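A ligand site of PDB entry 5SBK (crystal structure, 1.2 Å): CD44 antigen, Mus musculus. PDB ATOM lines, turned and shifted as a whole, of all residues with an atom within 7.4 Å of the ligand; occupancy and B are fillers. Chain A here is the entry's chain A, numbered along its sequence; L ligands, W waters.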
ATOM      1  N   THR A   9       6.158  14.132   7.923  1.00  0.00           N
ATOM      2  CA  THR A   9       5.181  14.879   7.161  1.00  0.00           C
ATOM      3  C   THR A   9       4.519  15.969   8.030  1.00  0.00           C
ATOM      4  O   THR A   9       4.747  16.057   9.243  1.00  0.00           O
ATOM      5  CB  THR A   9       4.075  13.906   6.643  1.00  0.00           C
ATOM      6  OG1 THR A   9       3.368  13.331   7.762  1.00  0.00           O
ATOM      7  CG2 THR A   9       4.591  12.834   5.740  1.00  0.00           C
ATOM      8  N   ARG A  11       1.265  17.127  10.122  1.00  0.00           N
ATOM      9  CA  ARG A  11       0.408  16.419  11.033  1.00  0.00           C
ATOM     10  C   ARG A  11      -1.017  16.739  10.641  1.00  0.00           C
ATOM     11  O   ARG A  11      -1.347  17.887  10.328  1.00  0.00           O
ATOM     12  CB  ARG A  11       0.663  16.831  12.489  1.00  0.00           C
ATOM     13  CG  ARG A  11       1.863  16.134  13.155  1.00  0.00           C
ATOM     14  CD  ARG A  11       3.185  16.568  12.554  1.00  0.00           C
ATOM     15  NE  ARG A  11       3.383  17.971  12.844  1.00  0.00           N
ATOM     16  CZ  ARG A  11       3.952  18.849  12.034  1.00  0.00           C
ATOM     17  NH1 ARG A  11       4.489  18.477  10.873  1.00  0.00           N
ATOM     18  NH2 ARG A  11       4.020  20.122  12.387  1.00  0.00           N
ATOM     19  N   GLY A  14      -3.046  15.491  14.479  1.00  0.00           N
ATOM     20  CA  GLY A  14      -1.940  14.912  15.250  1.00  0.00           C
ATOM     21  C   GLY A  14      -1.261  13.716  14.638  1.00  0.00           C
ATOM     22  O   GLY A  14      -0.298  13.228  15.201  1.00  0.00           O
ATOM     23  N   PHE A  16       0.946  11.786  11.827  1.00  0.00           N
ATOM     24  CA  PHE A  16       1.945  12.077  10.796  1.00  0.00           C
ATOM     25  C   PHE A  16       2.658  10.801  10.404  1.00  0.00           C
ATOM     26  O   PHE A  16       2.536   9.788  11.078  1.00  0.00           O
ATOM     27  CB  PHE A  16       2.983  13.117  11.261  1.00  0.00           C
ATOM     28  CG  PHE A  16       3.782  12.789  12.523  1.00  0.00           C
ATOM     29  CD1 PHE A  16       3.177  12.787  13.766  1.00  0.00           C
ATOM     30  CD2 PHE A  16       5.143  12.548  12.459  1.00  0.00           C
ATOM     31  CE1 PHE A  16       3.914  12.534  14.935  1.00  0.00           C
ATOM     32  CE2 PHE A  16       5.893  12.338  13.622  1.00  0.00           C
ATOM     33  CZ  PHE A  16       5.264  12.298  14.841  1.00  0.00           C
ATOM     34  N   CYS A  35       7.787   6.433  17.755  1.00  0.00           N
ATOM     35  CA  CYS A  35       6.700   7.374  18.080  1.00  0.00           C
ATOM     36  C   CYS A  35       6.865   7.894  19.482  1.00  0.00           C
ATOM     37  O   CYS A  35       6.682   9.090  19.678  1.00  0.00           O
ATOM     38  CB  CYS A  35       5.338   6.710  17.918  1.00  0.00           C
ATOM     39  SG  CYS A  35       4.934   6.305  16.208  1.00  0.00           S
ATOM     40  N   ALA A  37       9.580   8.545  21.018  1.00  0.00           N
ATOM     41  CA  ALA A  37      10.598   9.595  20.969  1.00  0.00           C
ATOM     42  C   ALA A  37      10.004  10.944  20.483  1.00  0.00           C
ATOM     43  O   ALA A  37      10.512  12.005  20.786  1.00  0.00           O
ATOM     44  CB  ALA A  37      11.773   9.164  20.097  1.00  0.00           C
ATOM     45  N   PHE A  38       8.927  10.894  19.707  1.00  0.00           N
ATOM     46  CA  PHE A  38       8.206  12.055  19.259  1.00  0.00           C
ATOM     47  C   PHE A  38       7.076  12.404  20.265  1.00  0.00           C
ATOM     48  O   PHE A  38       6.176  13.135  19.891  1.00  0.00           O
ATOM     49  CB  PHE A  38       7.576  11.804  17.871  1.00  0.00           C
ATOM     50  CG  PHE A  38       8.530  11.900  16.719  1.00  0.00           C
ATOM     51  CD1 PHE A  38       9.003  13.123  16.282  1.00  0.00           C
ATOM     52  CD2 PHE A  38       8.932  10.753  16.028  1.00  0.00           C
ATOM     53  CE1 PHE A  38       9.851  13.213  15.189  1.00  0.00           C
ATOM     54  CE2 PHE A  38       9.793  10.831  14.950  1.00  0.00           C
ATOM     55  CZ  PHE A  38      10.248  12.059  14.540  1.00  0.00           C
ATOM     56  N   ASN A  39       7.087  11.843  21.514  1.00  0.00           N
ATOM     57  CA  ASN A  39       6.004  12.063  22.516  1.00  0.00           C
ATOM     58  C   ASN A  39       4.657  11.677  21.886  1.00  0.00           C
ATOM     59  O   ASN A  39       3.649  12.347  22.046  1.00  0.00           O
ATOM     60  CB  ASN A  39       5.956  13.529  22.950  1.00  0.00           C
ATOM     61  CG  ASN A  39       6.924  13.937  24.020  1.00  0.00           C
ATOM     62  OD1 ASN A  39       7.364  15.089  24.079  1.00  0.00           O
ATOM     63  ND2 ASN A  39       7.222  13.039  24.912  1.00  0.00           N
ATOM     64  N   SER A  40       4.679  10.560  21.145  1.00  0.00           N
ATOM     65  CA  SER A  40       3.569  10.161  20.322  1.00  0.00           C
ATOM     66  C   SER A  40       3.371   8.666  20.485  1.00  0.00           C
ATOM     67  O   SER A  40       4.133   7.970  21.183  1.00  0.00           O
ATOM     68  CB  SER A  40       3.881  10.513  18.858  1.00  0.00           C
ATOM     69  OG  SER A  40       4.041  11.897  18.620  1.00  0.00           O
ATOM     70  N   CYS A 101       2.579   8.095  13.429  1.00  0.00           N
ATOM     71  CA  CYS A 101       2.605   8.439  14.856  1.00  0.00           C
ATOM     72  C   CYS A 101       1.505   9.436  15.096  1.00  0.00           C
ATOM     73  O   CYS A 101       1.048  10.110  14.159  1.00  0.00           O
ATOM     74  CB  CYS A 101       3.942   9.060  15.253  1.00  0.00           C
ATOM     75  SG  CYS A 101       5.355   7.951  15.106  1.00  0.00           S
ATOM     76  N   PHE A 102       1.018   9.478  16.353  1.00  0.00           N
ATOM     77  CA  PHE A 102      -0.040  10.410  16.745  1.00  0.00           C
ATOM     78  C   PHE A 102       0.446  11.198  17.935  1.00  0.00           C
ATOM     79  O   PHE A 102       0.842  10.622  18.934  1.00  0.00           O
ATOM     80  CB  PHE A 102      -1.303   9.581  17.127  1.00  0.00           C
ATOM     81  CG  PHE A 102      -2.283  10.457  17.849  1.00  0.00           C
ATOM     82  CD1 PHE A 102      -2.911  11.498  17.194  1.00  0.00           C
ATOM     83  CD2 PHE A 102      -2.503  10.294  19.198  1.00  0.00           C
ATOM     84  CE1 PHE A 102      -3.778  12.337  17.871  1.00  0.00           C
ATOM     85  CE2 PHE A 102      -3.356  11.143  19.879  1.00  0.00           C
ATOM     86  CZ  PHE A 102      -3.975  12.156  19.212  1.00  0.00           C
ATOM     87  N   ASN A 103       0.454  12.525  17.799  1.00  0.00           N
ATOM     88  CA  ASN A 103       0.802  13.410  18.920  1.00  0.00           C
ATOM     89  C   ASN A 103      -0.459  14.185  19.326  1.00  0.00           C
ATOM     90  O   ASN A 103      -0.992  14.962  18.530  1.00  0.00           O
ATOM     91  CB  ASN A 103       1.905  14.386  18.519  1.00  0.00           C
ATOM     92  CG  ASN A 103       2.386  15.165  19.700  1.00  0.00           C
ATOM     93  OD1 ASN A 103       1.631  15.902  20.298  1.00  0.00           O
ATOM     94  ND2 ASN A 103       3.609  15.000  20.134  1.00  0.00           N
ATOM     95  N   ALA A 104      -0.946  13.949  20.546  1.00  0.00           N
ATOM     96  CA  ALA A 104      -2.168  14.561  21.026  1.00  0.00           C
ATOM     97  C   ALA A 104      -2.106  16.052  21.180  1.00  0.00           C
ATOM     98  O   ALA A 104      -3.170  16.682  21.211  1.00  0.00           O
ATOM     99  CB  ALA A 104      -2.561  13.915  22.346  1.00  0.00           C
ATOM    100  N   SER A 105      -0.908  16.655  21.299  1.00  0.00           N
ATOM    101  CA  SER A 105      -0.793  18.111  21.496  1.00  0.00           C
ATOM    102  C   SER A 105      -0.708  18.896  20.212  1.00  0.00           C
ATOM    103  O   SER A 105      -0.568  20.128  20.253  1.00  0.00           O
ATOM    104  CB  SER A 105       0.432  18.442  22.334  1.00  0.00           C
ATOM    105  OG  SER A 105       0.323  17.738  23.558  1.00  0.00           O
ATOM    106  N   ALA A 106      -0.716  18.220  19.051  1.00  0.00           N
ATOM    107  CA  ALA A 106      -0.646  18.866  17.746  1.00  0.00           C
ATOM    108  C   ALA A 106      -1.977  19.577  17.474  1.00  0.00           C
ATOM    109  O   ALA A 106      -2.971  19.341  18.147  1.00  0.00           O
ATOM    110  CB  ALA A 106      -0.367  17.792  16.673  1.00  0.00           C
ATOM    111  N   PRO A 107      -2.040  20.457  16.467  1.00  0.00           N
ATOM    112  CA  PRO A 107      -3.315  21.126  16.157  1.00  0.00           C
ATOM    113  C   PRO A 107      -4.399  20.122  15.708  1.00  0.00           C
ATOM    114  O   PRO A 107      -4.090  19.019  15.254  1.00  0.00           O
ATOM    115  CB  PRO A 107      -2.956  22.100  15.039  1.00  0.00           C
ATOM    116  CG  PRO A 107      -1.441  22.330  15.173  1.00  0.00           C
ATOM    117  CD  PRO A 107      -0.947  20.955  15.607  1.00  0.00           C
ATOM    118  N   ASP A 111      -1.711  20.625   9.988  1.00  0.00           N
ATOM    119  CA  ASP A 111      -0.583  21.377  10.496  1.00  0.00           C
ATOM    120  C   ASP A 111       0.596  21.039   9.620  1.00  0.00           C
ATOM    121  O   ASP A 111       1.261  19.977   9.776  1.00  0.00           O
ATOM    122  CB  ASP A 111      -0.254  21.020  11.955  1.00  0.00           C
ATOM    123  CG  ASP A 111       0.975  21.726  12.465  1.00  0.00           C
ATOM    124  OD1 ASP A 111       1.423  22.713  11.807  1.00  0.00           O
ATOM    125  OD2 ASP A 111       1.493  21.318  13.530  1.00  0.00           O
ATOM    126  N   CYS A 112       0.876  21.919   8.657  1.00  0.00           N
ATOM    127  CA  CYS A 112       1.985  21.716   7.741  1.00  0.00           C
ATOM    128  C   CYS A 112       3.170  22.614   8.079  1.00  0.00           C
ATOM    129  O   CYS A 112       3.957  22.979   7.191  1.00  0.00           O
ATOM    130  CB  CYS A 112       1.533  21.840   6.297  1.00  0.00           C
ATOM    131  SG  CYS A 112       0.600  20.389   5.717  1.00  0.00           S
ATOM    132  N   THR A 113       3.323  22.946   9.387  1.00  0.00           N
ATOM    133  CA  THR A 113       4.556  23.553   9.829  1.00  0.00           C
ATOM    134  C   THR A 113       5.541  22.382   9.956  1.00  0.00           C
ATOM    135  O   THR A 113       5.152  21.190   9.902  1.00  0.00           O
ATOM    136  CB  THR A 113       4.364  24.287  11.174  1.00  0.00           C
ATOM    137  OG1 THR A 113       3.930  23.308  12.131  1.00  0.00           O
ATOM    138  CG2 THR A 113       3.382  25.442  11.080  1.00  0.00           C
ATOM    139  N   SER A 114       6.803  22.696  10.165  1.00  0.00           N
ATOM    140  CA  SER A 114       7.808  21.643  10.266  1.00  0.00           C
ATOM    141  C   SER A 114       7.894  21.036  11.682  1.00  0.00           C
ATOM    142  O   SER A 114       7.491  21.662  12.666  1.00  0.00           O
ATOM    143  CB  SER A 114       9.151  22.202   9.821  1.00  0.00           C
ATOM    144  OG  SER A 114       9.407  23.398  10.541  1.00  0.00           O
ATOM    145  N   VAL A 115       8.430  19.828  11.768  1.00  0.00           N
ATOM    146  CA  VAL A 115       8.707  19.170  13.021  1.00  0.00           C
ATOM    147  C   VAL A 115      10.116  19.668  13.381  1.00  0.00           C
ATOM    148  O   VAL A 115      11.052  19.612  12.561  1.00  0.00           O
ATOM    149  CB  VAL A 115       8.673  17.657  12.880  1.00  0.00           C
ATOM    150  CG1 VAL A 115       9.145  17.002  14.169  1.00  0.00           C
ATOM    151  CG2 VAL A 115       7.274  17.227  12.533  1.00  0.00           C
ATOM    152  N   THR A 116      10.260  20.212  14.583  1.00  0.00           N
ATOM    153  CA  THR A 116      11.495  20.876  14.992  1.00  0.00           C
ATOM    154  C   THR A 116      12.144  20.252  16.219  1.00  0.00           C
ATOM    155  O   THR A 116      13.067  20.855  16.757  1.00  0.00           O
ATOM    156  CB  THR A 116      11.188  22.347  15.262  1.00  0.00           C
ATOM    157  OG1 THR A 116      10.214  22.394  16.293  1.00  0.00           O
ATOM    158  CG2 THR A 116      10.640  23.065  14.056  1.00  0.00           C
ATOM    159  N   ASP A 117      11.707  19.063  16.645  1.00  0.00           N
ATOM    160  CA  ASP A 117      12.309  18.398  17.802  1.00  0.00           C
ATOM    161  C   ASP A 117      11.901  16.931  17.803  1.00  0.00           C
ATOM    162  O   ASP A 117      10.928  16.528  17.152  1.00  0.00           O
ATOM    163  CB  ASP A 117      11.845  19.073  19.114  1.00  0.00           C
ATOM    164  CG  ASP A 117      12.636  18.764  20.386  1.00  0.00           C
ATOM    165  OD1 ASP A 117      13.708  18.105  20.292  1.00  0.00           O
ATOM    166  OD2 ASP A 117      12.184  19.172  21.483  1.00  0.00           O
ATOM    167  N   LEU A 118      12.647  16.134  18.552  1.00  0.00           N
ATOM    168  CA  LEU A 118      12.416  14.723  18.858  1.00  0.00           C
ATOM    169  C   LEU A 118      12.466  14.817  20.385  1.00  0.00           C
ATOM    170  O   LEU A 118      13.535  14.632  20.994  1.00  0.00           O
ATOM    171  CB  LEU A 118      13.593  13.926  18.323  1.00  0.00           C
ATOM    172  CG  LEU A 118      13.485  12.423  18.386  1.00  0.00           C
ATOM    173  CD1 LEU A 118      12.297  11.914  17.585  1.00  0.00           C
ATOM    174  CD2 LEU A 118      14.746  11.778  17.882  1.00  0.00           C
ATOM    175  N   PRO A 119      11.362  15.266  21.008  1.00  0.00           N
ATOM    176  CA  PRO A 119      11.423  15.677  22.414  1.00  0.00           C
ATOM    177  C   PRO A 119      11.717  14.622  23.443  1.00  0.00           C
ATOM    178  O   PRO A 119      12.171  14.957  24.546  1.00  0.00           O
ATOM    179  CB  PRO A 119      10.043  16.292  22.662  1.00  0.00           C
ATOM    180  CG  PRO A 119       9.169  15.722  21.557  1.00  0.00           C
ATOM    181  CD  PRO A 119      10.067  15.622  20.399  1.00  0.00           C
ATOM    182  N   ILE A 130      15.846  14.793  11.814  1.00  0.00           N
ATOM    183  CA  ILE A 130      14.486  14.875  11.349  1.00  0.00           C
ATOM    184  C   ILE A 130      14.541  15.677  10.079  1.00  0.00           C
ATOM    185  O   ILE A 130      15.088  16.806  10.074  1.00  0.00           O
ATOM    186  CB  ILE A 130      13.564  15.579  12.364  1.00  0.00           C
ATOM    187  CG1 ILE A 130      13.364  14.722  13.615  1.00  0.00           C
ATOM    188  CG2 ILE A 130      12.229  15.958  11.726  1.00  0.00           C
ATOM    189  CD1 ILE A 130      13.113  15.518  14.770  1.00  0.00           C
ATOM    190  N   ASN A 132      12.235  17.374   7.209  1.00  0.00           N
ATOM    191  CA  ASN A 132      10.910  17.786   6.788  1.00  0.00           C
ATOM    192  C   ASN A 132      10.742  17.732   5.284  1.00  0.00           C
ATOM    193  O   ASN A 132      11.733  17.686   4.537  1.00  0.00           O
ATOM    194  CB  ASN A 132      10.615  19.207   7.339  1.00  0.00           C
ATOM    195  CG  ASN A 132      10.372  19.145   8.798  1.00  0.00           C
ATOM    196  OD1 ASN A 132       9.281  18.732   9.240  1.00  0.00           O
ATOM    197  ND2 ASN A 132      11.390  19.410   9.601  1.00  0.00           N
HETATM  198  C1  LIG L   1       6.444  17.846  16.754  1.00  0.00           C
HETATM  199  C2  LIG L   1       5.482  15.338  17.232  1.00  0.00           C
HETATM  200  C3  LIG L   1       5.310  17.398  16.085  1.00  0.00           C
HETATM  201  O1  LIG L   1       8.110  19.484  16.349  1.00  0.00           O
HETATM  202  C4  LIG L   1       6.951  19.238  16.467  1.00  0.00           C
HETATM  203  N1  LIG L   1       5.951  20.247  16.330  1.00  0.00           N
HETATM  204  C5  LIG L   1       6.373  21.561  15.998  1.00  0.00           C
HETATM  205  C6  LIG L   1       6.363  22.452  17.204  1.00  0.00           C
HETATM  206  C7  LIG L   1       6.514  23.889  16.837  1.00  0.00           C
HETATM  207  C8  LIG L   1       5.479  24.337  15.796  1.00  0.00           C
HETATM  208  N2  LIG L   1       5.292  23.394  14.652  1.00  0.00           N
HETATM  209  C9  LIG L   1       5.350  21.931  14.936  1.00  0.00           C
HETATM  210  C10 LIG L   1       7.127  17.066  17.673  1.00  0.00           C
HETATM  211  C11 LIG L   1       6.607  15.805  17.910  1.00  0.00           C
HETATM  212  C12 LIG L   1       4.814  16.109  16.312  1.00  0.00           C
HETATM  213  O   HOH W   1       7.549  24.379  13.185  1.00  0.00           O
HETATM  214  O   HOH W   2       2.281  23.561  15.089  1.00  0.00           O
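N of Ser 105 sits at hydrogen-bond distance from OD1 of Asn 103 (2.8 Å). The side-chain sulfur of Cys 101 forms a disulfide with the side-chain sulfur of Cys 35 (2.0 Å). N of Asn 103 is in hydrogen-bond range of O of Gly 14 (2.8 Å). N of Val 115 lies within hydrogen-bond range of OD1 of Asn 132. The backbone carbonyl oxygen (O) of Phe 38 is in hydrogen-bond range of the side-chain amide nitrogen (ND2) of Asn 103 (3.2 Å). OG1 of Thr 113 sits at hydrogen-bond distance from OD1 of Asp 111 (2.6 Å). O of Cys 35 is in hydrogen-bond range of N of Ser 40 (2.9 Å). ND2 of Asn 103 sits at hydrogen-bond distance from O of Asn 39 (3.3 Å).
Water W1 lies within hydrogen-bond range of O of Ser 114 (2.8 Å) and N2 of the ligand (2.9 Å). Water W2 lies within hydrogen-bond range of the side-chain carboxylate of Asp 111 (2.8 Å), a nitrogen (N2) of the ligand (3.0 Å) and the side-chain hydroxyl of Thr 113 (3.4 Å).
O of Ser 114 sits close to N2 of the ligand, at 3.4 Å. The side-chain hydroxyl (OG1) of Thr 113 lies within hydrogen-bond range of a nitrogen (N2) of the ligand. The backbone NH (N) of Thr 116 sits at hydrogen-bond distance from an oxygen (O1) of the ligand (2.9 Å).
Merely in contact with the ligand: Phe 38, Val 115, Arg 11, Asn 103, Asp 117, Phe 16 and Ser 40. Hydrophobic or aromatic side chains that line the ligand: Phe 16, Phe 38 and Val 115. The nearest printed residue that does not touch the ligand is Asp 111 (4.2 Å).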
